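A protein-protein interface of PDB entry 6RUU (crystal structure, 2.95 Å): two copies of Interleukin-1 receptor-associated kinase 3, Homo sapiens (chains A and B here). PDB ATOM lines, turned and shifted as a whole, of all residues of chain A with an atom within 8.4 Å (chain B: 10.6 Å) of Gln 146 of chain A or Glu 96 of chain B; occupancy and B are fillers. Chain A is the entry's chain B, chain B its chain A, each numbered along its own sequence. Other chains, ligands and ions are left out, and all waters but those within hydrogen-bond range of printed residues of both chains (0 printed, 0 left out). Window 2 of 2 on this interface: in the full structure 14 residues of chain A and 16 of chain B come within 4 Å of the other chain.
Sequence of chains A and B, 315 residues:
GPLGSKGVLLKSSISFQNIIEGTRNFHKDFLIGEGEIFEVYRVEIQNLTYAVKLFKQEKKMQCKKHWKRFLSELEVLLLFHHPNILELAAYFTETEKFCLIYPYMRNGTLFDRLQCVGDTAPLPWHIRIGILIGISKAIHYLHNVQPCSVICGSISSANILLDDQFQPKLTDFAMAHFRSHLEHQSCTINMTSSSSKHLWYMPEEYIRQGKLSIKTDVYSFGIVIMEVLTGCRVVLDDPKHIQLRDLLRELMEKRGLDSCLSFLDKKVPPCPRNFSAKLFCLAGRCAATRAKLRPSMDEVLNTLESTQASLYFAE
His 143 of chain A touches none of the printed residues of chain B.
No residue of chain B comes within 4 Å of Val 145 of chain A.
Of chain B, only Glu 96 comes within 4 Å of Gln 146 of chain A.
Pro 147 of chain A touches just these residues of chain B: Trp 67 and Phe 98.
Printed residues of chain A within 4 Å of Cys 63 of chain B: Cys 148 and Ser 180.
No residue of chain A comes within 4 Å of Thr 95 of chain B.
Of chain A, only Gln 146 comes within 4 Å of Glu 96 of chain B.
Of the printed residues of chain A, Phe 98 of chain B touches Pro 147.
Printed residues of chain B that touch a printed residue of chain A: Cys 63, Lys 64, Trp 67, Glu 96 and Phe 98.
Among the printed residues, 6 pairs touch across the chains.
Among the printed residues, no Asp or Glu carboxylate lies within 4 Å of a Lys or Arg side-chain nitrogen of the other chain.
Among the printed residues, merely in contact across the chains: Gln 146 of chain A with Glu 96 of chain B (3.2 Å), Pro 147 of chain A with Trp 67 of chain B (3.5 Å), Pro 147 of chain A with Phe 98 of chain B (3.2 Å), Ser 180 of chain A with Cys 63 of chain B (3.3 Å) and Ser 180 of chain A with Lys 64 of chain B (3.9 Å).
SG of Cys 63 of chain B forms a disulfide with SG of Cys 148 of chain A.
O of Phe 98 of chain B is in hydrogen-bond range of N of Phe 55 of chain B (3.0 Å).
No position is printed for both chains.
Of the 6 pairs that touch across the chains among the printed residues, none has its exchanged pair printed and touching as well.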
ATOM      1  N   PHE A  80      -4.423  -0.470 -18.264  1.00  0.00           N
ATOM      2  CA  PHE A  80      -5.263   0.591 -17.726  1.00  0.00           C
ATOM      3  C   PHE A  80      -5.995   1.279 -18.865  1.00  0.00           C
ATOM      4  O   PHE A  80      -5.381   1.651 -19.870  1.00  0.00           O
ATOM      5  CB  PHE A  80      -4.425   1.596 -16.933  1.00  0.00           C
ATOM      6  CG  PHE A  80      -3.661   0.974 -15.801  1.00  0.00           C
ATOM      7  CD1 PHE A  80      -4.295   0.635 -14.619  1.00  0.00           C
ATOM      8  CD2 PHE A  80      -2.304   0.719 -15.925  1.00  0.00           C
ATOM      9  CE1 PHE A  80      -3.591   0.052 -13.583  1.00  0.00           C
ATOM     10  CE2 PHE A  80      -1.596   0.142 -14.889  1.00  0.00           C
ATOM     11  CZ  PHE A  80      -2.240  -0.193 -13.717  1.00  0.00           C
ATOM     12  N   TYR A 141      -7.614   8.865 -12.081  1.00  0.00           N
ATOM     13  CA  TYR A 141      -7.732   7.425 -12.292  1.00  0.00           C
ATOM     14  C   TYR A 141      -6.390   6.719 -12.142  1.00  0.00           C
ATOM     15  O   TYR A 141      -6.301   5.678 -11.482  1.00  0.00           O
ATOM     16  CB  TYR A 141      -8.342   7.160 -13.670  1.00  0.00           C
ATOM     17  CG  TYR A 141      -8.225   5.734 -14.152  1.00  0.00           C
ATOM     18  CD1 TYR A 141      -8.962   4.713 -13.572  1.00  0.00           C
ATOM     19  CD2 TYR A 141      -7.389   5.416 -15.213  1.00  0.00           C
ATOM     20  CE1 TYR A 141      -8.851   3.409 -14.025  1.00  0.00           C
ATOM     21  CE2 TYR A 141      -7.273   4.122 -15.672  1.00  0.00           C
ATOM     22  CZ  TYR A 141      -8.004   3.122 -15.078  1.00  0.00           C
ATOM     23  OH  TYR A 141      -7.884   1.833 -15.542  1.00  0.00           O
ATOM     24  N   LEU A 142      -5.329   7.280 -12.727  1.00  0.00           N
ATOM     25  CA  LEU A 142      -4.032   6.610 -12.687  1.00  0.00           C
ATOM     26  C   LEU A 142      -3.416   6.678 -11.293  1.00  0.00           C
ATOM     27  O   LEU A 142      -2.783   5.716 -10.844  1.00  0.00           O
ATOM     28  CB  LEU A 142      -3.085   7.217 -13.722  1.00  0.00           C
ATOM     29  CG  LEU A 142      -3.214   6.806 -15.195  1.00  0.00           C
ATOM     30  CD1 LEU A 142      -3.122   5.306 -15.384  1.00  0.00           C
ATOM     31  CD2 LEU A 142      -4.473   7.328 -15.820  1.00  0.00           C
ATOM     32  N   HIS A 143      -3.588   7.800 -10.591  1.00  0.00           N
ATOM     33  CA  HIS A 143      -3.058   7.918  -9.236  1.00  0.00           C
ATOM     34  C   HIS A 143      -3.734   6.991  -8.235  1.00  0.00           C
ATOM     35  O   HIS A 143      -3.231   6.858  -7.115  1.00  0.00           O
ATOM     36  CB  HIS A 143      -3.175   9.354  -8.719  1.00  0.00           C
ATOM     37  CG  HIS A 143      -2.115  10.281  -9.227  1.00  0.00           C
ATOM     38  ND1 HIS A 143      -2.258  11.031 -10.374  1.00  0.00           N
ATOM     39  CD2 HIS A 143      -0.896  10.592  -8.726  1.00  0.00           C
ATOM     40  CE1 HIS A 143      -1.170  11.757 -10.561  1.00  0.00           C
ATOM     41  NE2 HIS A 143      -0.328  11.509  -9.575  1.00  0.00           N
ATOM     42  N   ASN A 144      -4.848   6.359  -8.588  1.00  0.00           N
ATOM     43  CA  ASN A 144      -5.560   5.501  -7.649  1.00  0.00           C
ATOM     44  C   ASN A 144      -5.901   4.159  -8.278  1.00  0.00           C
ATOM     45  O   ASN A 144      -7.007   3.637  -8.111  1.00  0.00           O
ATOM     46  CB  ASN A 144      -6.817   6.189  -7.128  1.00  0.00           C
ATOM     47  CG  ASN A 144      -6.504   7.432  -6.327  1.00  0.00           C
ATOM     48  OD1 ASN A 144      -6.876   8.539  -6.710  1.00  0.00           O
ATOM     49  ND2 ASN A 144      -5.800   7.258  -5.215  1.00  0.00           N
ATOM     50  N   VAL A 145      -4.957   3.573  -9.006  1.00  0.00           N
ATOM     51  CA  VAL A 145      -5.151   2.226  -9.524  1.00  0.00           C
ATOM     52  C   VAL A 145      -4.832   1.221  -8.428  1.00  0.00           C
ATOM     53  O   VAL A 145      -3.958   1.441  -7.579  1.00  0.00           O
ATOM     54  CB  VAL A 145      -4.307   1.980 -10.787  1.00  0.00           C
ATOM     55  CG1 VAL A 145      -4.768   2.886 -11.911  1.00  0.00           C
ATOM     56  CG2 VAL A 145      -2.837   2.187 -10.492  1.00  0.00           C
ATOM     57  N   GLN A 146      -5.546   0.097  -8.464  1.00  0.00           N
ATOM     58  CA  GLN A 146      -5.560  -0.835  -7.337  1.00  0.00           C
ATOM     59  C   GLN A 146      -4.205  -1.451  -7.012  1.00  0.00           C
ATOM     60  O   GLN A 146      -3.828  -1.446  -5.827  1.00  0.00           O
ATOM     61  CB  GLN A 146      -6.604  -1.921  -7.602  1.00  0.00           C
ATOM     62  N   PRO A 147      -3.437  -2.022  -7.973  1.00  0.00           N
ATOM     63  CA  PRO A 147      -2.207  -2.731  -7.585  1.00  0.00           C
ATOM     64  C   PRO A 147      -1.228  -1.824  -6.869  1.00  0.00           C
ATOM     65  O   PRO A 147      -0.886  -2.032  -5.701  1.00  0.00           O
ATOM     66  CB  PRO A 147      -1.616  -3.186  -8.927  1.00  0.00           C
ATOM     67  CG  PRO A 147      -2.712  -3.102  -9.882  1.00  0.00           C
ATOM     68  CD  PRO A 147      -3.585  -1.981  -9.437  1.00  0.00           C
ATOM     69  N   CYS A 148      -0.813  -0.784  -7.586  1.00  0.00           N
ATOM     70  CA  CYS A 148       0.195   0.164  -7.136  1.00  0.00           C
ATOM     71  C   CYS A 148       0.008   1.427  -7.964  1.00  0.00           C
ATOM     72  O   CYS A 148      -0.028   1.352  -9.195  1.00  0.00           O
ATOM     73  CB  CYS A 148       1.612  -0.407  -7.311  1.00  0.00           C
ATOM     74  SG  CYS A 148       2.021  -1.855  -6.276  1.00  0.00           S
ATOM     75  N   SER A 149      -0.131   2.571  -7.296  1.00  0.00           N
ATOM     76  CA  SER A 149      -0.441   3.808  -8.005  1.00  0.00           C
ATOM     77  C   SER A 149       0.649   4.137  -9.018  1.00  0.00           C
ATOM     78  O   SER A 149       1.838   3.915  -8.772  1.00  0.00           O
ATOM     79  CB  SER A 149      -0.612   4.961  -7.013  1.00  0.00           C
ATOM     80  OG  SER A 149       0.601   5.253  -6.345  1.00  0.00           O
ATOM     81  N   VAL A 150       0.233   4.664 -10.169  1.00  0.00           N
ATOM     82  CA  VAL A 150       1.133   4.970 -11.277  1.00  0.00           C
ATOM     83  C   VAL A 150       1.200   6.478 -11.472  1.00  0.00           C
ATOM     84  O   VAL A 150       0.180   7.174 -11.405  1.00  0.00           O
ATOM     85  CB  VAL A 150       0.694   4.255 -12.573  1.00  0.00           C
ATOM     86  CG1 VAL A 150      -0.687   4.679 -12.968  1.00  0.00           C
ATOM     87  CG2 VAL A 150       1.665   4.551 -13.701  1.00  0.00           C
ATOM     88  N   ARG A 179       4.266   3.562  -7.972  1.00  0.00           N
ATOM     89  CA  ARG A 179       4.759   4.148  -6.730  1.00  0.00           C
ATOM     90  C   ARG A 179       4.085   3.537  -5.511  1.00  0.00           C
ATOM     91  O   ARG A 179       2.854   3.434  -5.466  1.00  0.00           O
ATOM     92  CB  ARG A 179       4.549   5.668  -6.725  1.00  0.00           C
ATOM     93  N   SER A 180       4.909   3.137  -4.540  1.00  0.00           N
ATOM     94  CA  SER A 180       4.511   2.840  -3.159  1.00  0.00           C
ATOM     95  C   SER A 180       5.717   2.314  -2.387  1.00  0.00           C
ATOM     96  O   SER A 180       6.368   1.360  -2.815  1.00  0.00           O
ATOM     97  CB  SER A 180       3.370   1.828  -3.083  1.00  0.00           C
ATOM     98  N   PHE B  16     -12.908 -13.244 -18.502  1.00  0.00           N
ATOM     99  CA  PHE B  16     -12.645 -13.306 -17.066  1.00  0.00           C
ATOM    100  C   PHE B  16     -13.823 -13.899 -16.305  1.00  0.00           C
ATOM    101  O   PHE B  16     -13.639 -14.469 -15.223  1.00  0.00           O
ATOM    102  CB  PHE B  16     -12.311 -11.915 -16.525  1.00  0.00           C
ATOM    103  CG  PHE B  16     -12.054 -11.886 -15.043  1.00  0.00           C
ATOM    104  CD1 PHE B  16     -10.876 -12.391 -14.520  1.00  0.00           C
ATOM    105  CD2 PHE B  16     -12.991 -11.350 -14.174  1.00  0.00           C
ATOM    106  CE1 PHE B  16     -10.639 -12.366 -13.157  1.00  0.00           C
ATOM    107  CE2 PHE B  16     -12.759 -11.321 -12.811  1.00  0.00           C
ATOM    108  CZ  PHE B  16     -11.581 -11.830 -12.302  1.00  0.00           C
ATOM    109  N   GLN B  17     -15.036 -13.769 -16.843  1.00  0.00           N
ATOM    110  CA  GLN B  17     -16.180 -14.420 -16.218  1.00  0.00           C
ATOM    111  C   GLN B  17     -16.055 -15.938 -16.284  1.00  0.00           C
ATOM    112  O   GLN B  17     -16.519 -16.636 -15.376  1.00  0.00           O
ATOM    113  CB  GLN B  17     -17.477 -13.954 -16.880  1.00  0.00           C
ATOM    114  CG  GLN B  17     -17.775 -12.467 -16.694  1.00  0.00           C
ATOM    115  CD  GLN B  17     -17.999 -12.080 -15.240  1.00  0.00           C
ATOM    116  OE1 GLN B  17     -17.170 -11.406 -14.629  1.00  0.00           O
ATOM    117  NE2 GLN B  17     -19.130 -12.500 -14.684  1.00  0.00           N
ATOM    118  N   ILE B  20     -13.433 -16.915 -13.272  1.00  0.00           N
ATOM    119  CA  ILE B  20     -13.975 -16.839 -11.917  1.00  0.00           C
ATOM    120  C   ILE B  20     -14.918 -18.004 -11.642  1.00  0.00           C
ATOM    121  O   ILE B  20     -15.010 -18.482 -10.505  1.00  0.00           O
ATOM    122  CB  ILE B  20     -14.661 -15.473 -11.694  1.00  0.00           C
ATOM    123  CG1 ILE B  20     -14.989 -15.258 -10.214  1.00  0.00           C
ATOM    124  CG2 ILE B  20     -15.905 -15.332 -12.555  1.00  0.00           C
ATOM    125  CD1 ILE B  20     -13.772 -15.096  -9.335  1.00  0.00           C
ATOM    126  N   ASN B  25     -14.337 -18.810  -7.447  1.00  0.00           N
ATOM    127  CA  ASN B  25     -13.814 -17.666  -6.696  1.00  0.00           C
ATOM    128  C   ASN B  25     -12.430 -17.981  -6.134  1.00  0.00           C
ATOM    129  O   ASN B  25     -12.085 -17.594  -5.015  1.00  0.00           O
ATOM    130  CB  ASN B  25     -14.779 -17.237  -5.587  1.00  0.00           C
ATOM    131  CG  ASN B  25     -14.450 -15.865  -5.017  1.00  0.00           C
ATOM    132  OD1 ASN B  25     -13.493 -15.213  -5.438  1.00  0.00           O
ATOM    133  ND2 ASN B  25     -15.250 -15.421  -4.053  1.00  0.00           N
ATOM    134  N   PHE B  26     -11.638 -18.713  -6.921  1.00  0.00           N
ATOM    135  CA  PHE B  26     -10.258 -19.059  -6.590  1.00  0.00           C
ATOM    136  C   PHE B  26     -10.191 -19.845  -5.278  1.00  0.00           C
ATOM    137  O   PHE B  26      -9.491 -19.480  -4.329  1.00  0.00           O
ATOM    138  CB  PHE B  26      -9.381 -17.805  -6.539  1.00  0.00           C
ATOM    139  CG  PHE B  26      -9.318 -17.064  -7.845  1.00  0.00           C
ATOM    140  CD1 PHE B  26      -8.521 -17.521  -8.881  1.00  0.00           C
ATOM    141  CD2 PHE B  26     -10.059 -15.909  -8.036  1.00  0.00           C
ATOM    142  CE1 PHE B  26      -8.466 -16.840 -10.084  1.00  0.00           C
ATOM    143  CE2 PHE B  26     -10.007 -15.223  -9.237  1.00  0.00           C
ATOM    144  CZ  PHE B  26      -9.209 -15.691 -10.262  1.00  0.00           C
ATOM    145  N   LEU B  54      -2.370 -16.309 -10.877  1.00  0.00           N
ATOM    146  CA  LEU B  54      -2.943 -15.086 -10.335  1.00  0.00           C
ATOM    147  C   LEU B  54      -1.899 -14.323  -9.534  1.00  0.00           C
ATOM    148  O   LEU B  54      -1.091 -14.922  -8.820  1.00  0.00           O
ATOM    149  CB  LEU B  54      -4.145 -15.405  -9.442  1.00  0.00           C
ATOM    150  CG  LEU B  54      -4.937 -14.236  -8.849  1.00  0.00           C
ATOM    151  CD1 LEU B  54      -5.644 -13.444  -9.938  1.00  0.00           C
ATOM    152  CD2 LEU B  54      -5.930 -14.726  -7.806  1.00  0.00           C
ATOM    153  N   PHE B  55      -1.923 -12.998  -9.657  1.00  0.00           N
ATOM    154  CA  PHE B  55      -1.035 -12.161  -8.863  1.00  0.00           C
ATOM    155  C   PHE B  55      -1.369 -12.325  -7.385  1.00  0.00           C
ATOM    156  O   PHE B  55      -2.522 -12.165  -6.977  1.00  0.00           O
ATOM    157  CB  PHE B  55      -1.178 -10.695  -9.283  1.00  0.00           C
ATOM    158  CG  PHE B  55      -0.175  -9.771  -8.644  1.00  0.00           C
ATOM    159  CD1 PHE B  55       1.117  -9.685  -9.135  1.00  0.00           C
ATOM    160  CD2 PHE B  55      -0.521  -8.991  -7.552  1.00  0.00           C
ATOM    161  CE1 PHE B  55       2.042  -8.837  -8.555  1.00  0.00           C
ATOM    162  CE2 PHE B  55       0.403  -8.143  -6.965  1.00  0.00           C
ATOM    163  CZ  PHE B  55       1.686  -8.066  -7.468  1.00  0.00           C
ATOM    164  N   LYS B  56      -0.357 -12.653  -6.580  1.00  0.00           N
ATOM    165  CA  LYS B  56      -0.575 -12.782  -5.145  1.00  0.00           C
ATOM    166  C   LYS B  56      -0.783 -11.386  -4.577  1.00  0.00           C
ATOM    167  O   LYS B  56       0.182 -10.709  -4.203  1.00  0.00           O
ATOM    168  CB  LYS B  56       0.600 -13.488  -4.465  1.00  0.00           C
ATOM    169  CG  LYS B  56       0.384 -13.822  -2.999  1.00  0.00           C
ATOM    170  CD  LYS B  56       1.653 -14.390  -2.375  1.00  0.00           C
ATOM    171  CE  LYS B  56       1.931 -15.803  -2.857  1.00  0.00           C
ATOM    172  NZ  LYS B  56       3.098 -16.409  -2.157  1.00  0.00           N
ATOM    173  N   GLN B  57      -2.047 -10.955  -4.524  1.00  0.00           N
ATOM    174  CA  GLN B  57      -2.358  -9.545  -4.303  1.00  0.00           C
ATOM    175  C   GLN B  57      -1.812  -9.056  -2.968  1.00  0.00           C
ATOM    176  O   GLN B  57      -1.136  -8.022  -2.905  1.00  0.00           O
ATOM    177  CB  GLN B  57      -3.868  -9.330  -4.389  1.00  0.00           C
ATOM    178  CG  GLN B  57      -4.282  -7.876  -4.306  1.00  0.00           C
ATOM    179  CD  GLN B  57      -3.775  -7.067  -5.484  1.00  0.00           C
ATOM    180  OE1 GLN B  57      -3.797  -7.528  -6.625  1.00  0.00           O
ATOM    181  NE2 GLN B  57      -3.310  -5.854  -5.210  1.00  0.00           N
ATOM    182  N   GLU B  58      -2.094  -9.788  -1.891  1.00  0.00           N
ATOM    183  CA  GLU B  58      -1.536  -9.505  -0.567  1.00  0.00           C
ATOM    184  C   GLU B  58      -1.688  -8.042  -0.149  1.00  0.00           C
ATOM    185  O   GLU B  58      -0.730  -7.268  -0.208  1.00  0.00           O
ATOM    186  CB  GLU B  58      -0.057  -9.902  -0.524  1.00  0.00           C
ATOM    187  N   GLN B  62       6.638  -6.636  -1.073  1.00  0.00           N
ATOM    188  CA  GLN B  62       5.655  -5.560  -1.012  1.00  0.00           C
ATOM    189  C   GLN B  62       5.179  -5.155  -2.407  1.00  0.00           C
ATOM    190  O   GLN B  62       5.602  -5.734  -3.406  1.00  0.00           O
ATOM    191  CB  GLN B  62       6.240  -4.348  -0.283  1.00  0.00           C
ATOM    192  N   CYS B  63       4.304  -4.145  -2.445  1.00  0.00           N
ATOM    193  CA  CYS B  63       3.742  -3.599  -3.680  1.00  0.00           C
ATOM    194  C   CYS B  63       4.726  -3.503  -4.843  1.00  0.00           C
ATOM    195  O   CYS B  63       4.523  -4.122  -5.893  1.00  0.00           O
ATOM    196  CB  CYS B  63       3.165  -2.214  -3.362  1.00  0.00           C
ATOM    197  SG  CYS B  63       3.023  -1.015  -4.729  1.00  0.00           S
ATOM    198  N   LYS B  64       5.807  -2.741  -4.668  1.00  0.00           N
ATOM    199  CA  LYS B  64       6.627  -2.365  -5.816  1.00  0.00           C
ATOM    200  C   LYS B  64       7.395  -3.556  -6.378  1.00  0.00           C
ATOM    201  O   LYS B  64       7.530  -3.690  -7.601  1.00  0.00           O
ATOM    202  CB  LYS B  64       7.584  -1.238  -5.428  1.00  0.00           C
ATOM    203  N   TRP B  67       5.107  -6.279  -8.134  1.00  0.00           N
ATOM    204  CA  TRP B  67       4.486  -5.761  -9.346  1.00  0.00           C
ATOM    205  C   TRP B  67       5.469  -5.760 -10.511  1.00  0.00           C
ATOM    206  O   TRP B  67       5.108  -6.135 -11.631  1.00  0.00           O
ATOM    207  CB  TRP B  67       3.927  -4.362  -9.086  1.00  0.00           C
ATOM    208  CG  TRP B  67       3.147  -3.801 -10.231  1.00  0.00           C
ATOM    209  CD1 TRP B  67       3.493  -2.747 -11.027  1.00  0.00           C
ATOM    210  CD2 TRP B  67       1.904  -4.296 -10.736  1.00  0.00           C
ATOM    211  NE1 TRP B  67       2.525  -2.539 -11.981  1.00  0.00           N
ATOM    212  CE2 TRP B  67       1.541  -3.481 -11.825  1.00  0.00           C
ATOM    213  CE3 TRP B  67       1.057  -5.345 -10.367  1.00  0.00           C
ATOM    214  CZ2 TRP B  67       0.370  -3.682 -12.548  1.00  0.00           C
ATOM    215  CZ3 TRP B  67      -0.104  -5.543 -11.085  1.00  0.00           C
ATOM    216  CH2 TRP B  67      -0.438  -4.716 -12.163  1.00  0.00           C
ATOM    217  N   PHE B  70       5.641  -9.153 -11.976  1.00  0.00           N
ATOM    218  CA  PHE B  70       4.446  -9.397 -12.780  1.00  0.00           C
ATOM    219  C   PHE B  70       4.640  -8.905 -14.209  1.00  0.00           C
ATOM    220  O   PHE B  70       4.310  -9.603 -15.174  1.00  0.00           O
ATOM    221  CB  PHE B  70       3.237  -8.705 -12.147  1.00  0.00           C
ATOM    222  CG  PHE B  70       1.950  -8.917 -12.901  1.00  0.00           C
ATOM    223  CD1 PHE B  70       1.197 -10.063 -12.709  1.00  0.00           C
ATOM    224  CD2 PHE B  70       1.506  -7.982 -13.821  1.00  0.00           C
ATOM    225  CE1 PHE B  70       0.020 -10.263 -13.403  1.00  0.00           C
ATOM    226  CE2 PHE B  70       0.330  -8.182 -14.521  1.00  0.00           C
ATOM    227  CZ  PHE B  70      -0.412  -9.324 -14.310  1.00  0.00           C
ATOM    228  N   PHE B  92      -5.993 -10.874 -18.026  1.00  0.00           N
ATOM    229  CA  PHE B  92      -7.178 -10.135 -17.615  1.00  0.00           C
ATOM    230  C   PHE B  92      -6.834  -9.143 -16.513  1.00  0.00           C
ATOM    231  O   PHE B  92      -6.086  -9.459 -15.583  1.00  0.00           O
ATOM    232  CB  PHE B  92      -8.290 -11.088 -17.159  1.00  0.00           C
ATOM    233  CG  PHE B  92      -8.849 -11.929 -18.271  1.00  0.00           C
ATOM    234  CD1 PHE B  92      -9.759 -11.395 -19.168  1.00  0.00           C
ATOM    235  CD2 PHE B  92      -8.458 -13.247 -18.427  1.00  0.00           C
ATOM    236  CE1 PHE B  92     -10.274 -12.161 -20.199  1.00  0.00           C
ATOM    237  CE2 PHE B  92      -8.970 -14.019 -19.456  1.00  0.00           C
ATOM    238  CZ  PHE B  92      -9.880 -13.474 -20.342  1.00  0.00           C
ATOM    239  N   THR B  93      -7.398  -7.940 -16.633  1.00  0.00           N
ATOM    240  CA  THR B  93      -7.108  -6.823 -15.744  1.00  0.00           C
ATOM    241  C   THR B  93      -8.302  -6.377 -14.912  1.00  0.00           C
ATOM    242  O   THR B  93      -8.181  -5.406 -14.158  1.00  0.00           O
ATOM    243  CB  THR B  93      -6.594  -5.627 -16.557  1.00  0.00           C
ATOM    244  OG1 THR B  93      -6.260  -4.548 -15.676  1.00  0.00           O
ATOM    245  CG2 THR B  93      -7.651  -5.155 -17.548  1.00  0.00           C
ATOM    246  N   GLU B  94      -9.442  -7.051 -15.018  1.00  0.00           N
ATOM    247  CA  GLU B  94     -10.678  -6.551 -14.440  1.00  0.00           C
ATOM    248  C   GLU B  94     -10.838  -7.004 -12.990  1.00  0.00           C
ATOM    249  O   GLU B  94     -10.227  -7.978 -12.545  1.00  0.00           O
ATOM    250  CB  GLU B  94     -11.873  -7.010 -15.275  1.00  0.00           C
ATOM    251  CG  GLU B  94     -11.826  -6.522 -16.718  1.00  0.00           C
ATOM    252  CD  GLU B  94     -11.892  -5.009 -16.835  1.00  0.00           C
ATOM    253  OE1 GLU B  94     -12.557  -4.367 -15.994  1.00  0.00           O
ATOM    254  OE2 GLU B  94     -11.270  -4.460 -17.768  1.00  0.00           O
ATOM    255  N   THR B  95     -11.678  -6.267 -12.256  1.00  0.00           N
ATOM    256  CA  THR B  95     -11.968  -6.533 -10.842  1.00  0.00           C
ATOM    257  C   THR B  95     -10.709  -6.472  -9.980  1.00  0.00           C
ATOM    258  O   THR B  95     -10.569  -7.238  -9.025  1.00  0.00           O
ATOM    259  CB  THR B  95     -12.674  -7.879 -10.656  1.00  0.00           C
ATOM    260  N   GLU B  96      -9.783  -5.583 -10.346  1.00  0.00           N
ATOM    261  CA  GLU B  96      -8.467  -5.364  -9.740  1.00  0.00           C
ATOM    262  C   GLU B  96      -7.635  -6.639  -9.638  1.00  0.00           C
ATOM    263  O   GLU B  96      -6.554  -6.619  -9.038  1.00  0.00           O
ATOM    264  CB  GLU B  96      -8.537  -4.712  -8.346  1.00  0.00           C
ATOM    265  CG  GLU B  96      -8.895  -5.639  -7.195  1.00  0.00           C
ATOM    266  CD  GLU B  96      -8.790  -4.971  -5.839  1.00  0.00           C
ATOM    267  OE1 GLU B  96      -8.463  -3.767  -5.788  1.00  0.00           O
ATOM    268  OE2 GLU B  96      -9.018  -5.659  -4.823  1.00  0.00           O
ATOM    269  N   LYS B  97      -8.088  -7.744 -10.219  1.00  0.00           N
ATOM    270  CA  LYS B  97      -7.378  -9.010 -10.123  1.00  0.00           C
ATOM    271  C   LYS B  97      -6.657  -9.262 -11.439  1.00  0.00           C
ATOM    272  O   LYS B  97      -7.281  -9.273 -12.505  1.00  0.00           O
ATOM    273  CB  LYS B  97      -8.326 -10.158  -9.785  1.00  0.00           C
ATOM    274  CG  LYS B  97      -9.033  -9.978  -8.449  1.00  0.00           C
ATOM    275  CD  LYS B  97      -8.035  -9.829  -7.314  1.00  0.00           C
ATOM    276  CE  LYS B  97      -7.305 -11.128  -7.040  1.00  0.00           C
ATOM    277  NZ  LYS B  97      -6.360 -10.996  -5.896  1.00  0.00           N
ATOM    278  N   PHE B  98      -5.349  -9.451 -11.357  1.00  0.00           N
ATOM    279  CA  PHE B  98      -4.476  -9.539 -12.520  1.00  0.00           C
ATOM    280  C   PHE B  98      -3.999 -10.978 -12.631  1.00  0.00           C
ATOM    281  O   PHE B  98      -3.194 -11.437 -11.814  1.00  0.00           O
ATOM    282  CB  PHE B  98      -3.317  -8.560 -12.366  1.00  0.00           C
ATOM    283  CG  PHE B  98      -3.749  -7.127 -12.398  1.00  0.00           C
ATOM    284  CD1 PHE B  98      -3.738  -6.406 -13.579  1.00  0.00           C
ATOM    285  CD2 PHE B  98      -4.249  -6.527 -11.257  1.00  0.00           C
ATOM    286  CE1 PHE B  98      -4.156  -5.091 -13.602  1.00  0.00           C
ATOM    287  CE2 PHE B  98      -4.688  -5.227 -11.281  1.00  0.00           C
ATOM    288  CZ  PHE B  98      -4.636  -4.501 -12.452  1.00  0.00           C
ATOM    289  N   CYS B  99      -4.499 -11.687 -13.636  1.00  0.00           N
ATOM    290  CA  CYS B  99      -4.188 -13.096 -13.803  1.00  0.00           C
ATOM    291  C   CYS B  99      -3.712 -13.365 -15.222  1.00  0.00           C
ATOM    292  O   CYS B  99      -4.087 -12.671 -16.172  1.00  0.00           O
ATOM    293  CB  CYS B  99      -5.401 -13.981 -13.471  1.00  0.00           C
ATOM    294  SG  CYS B  99      -6.845 -13.705 -14.509  1.00  0.00           S
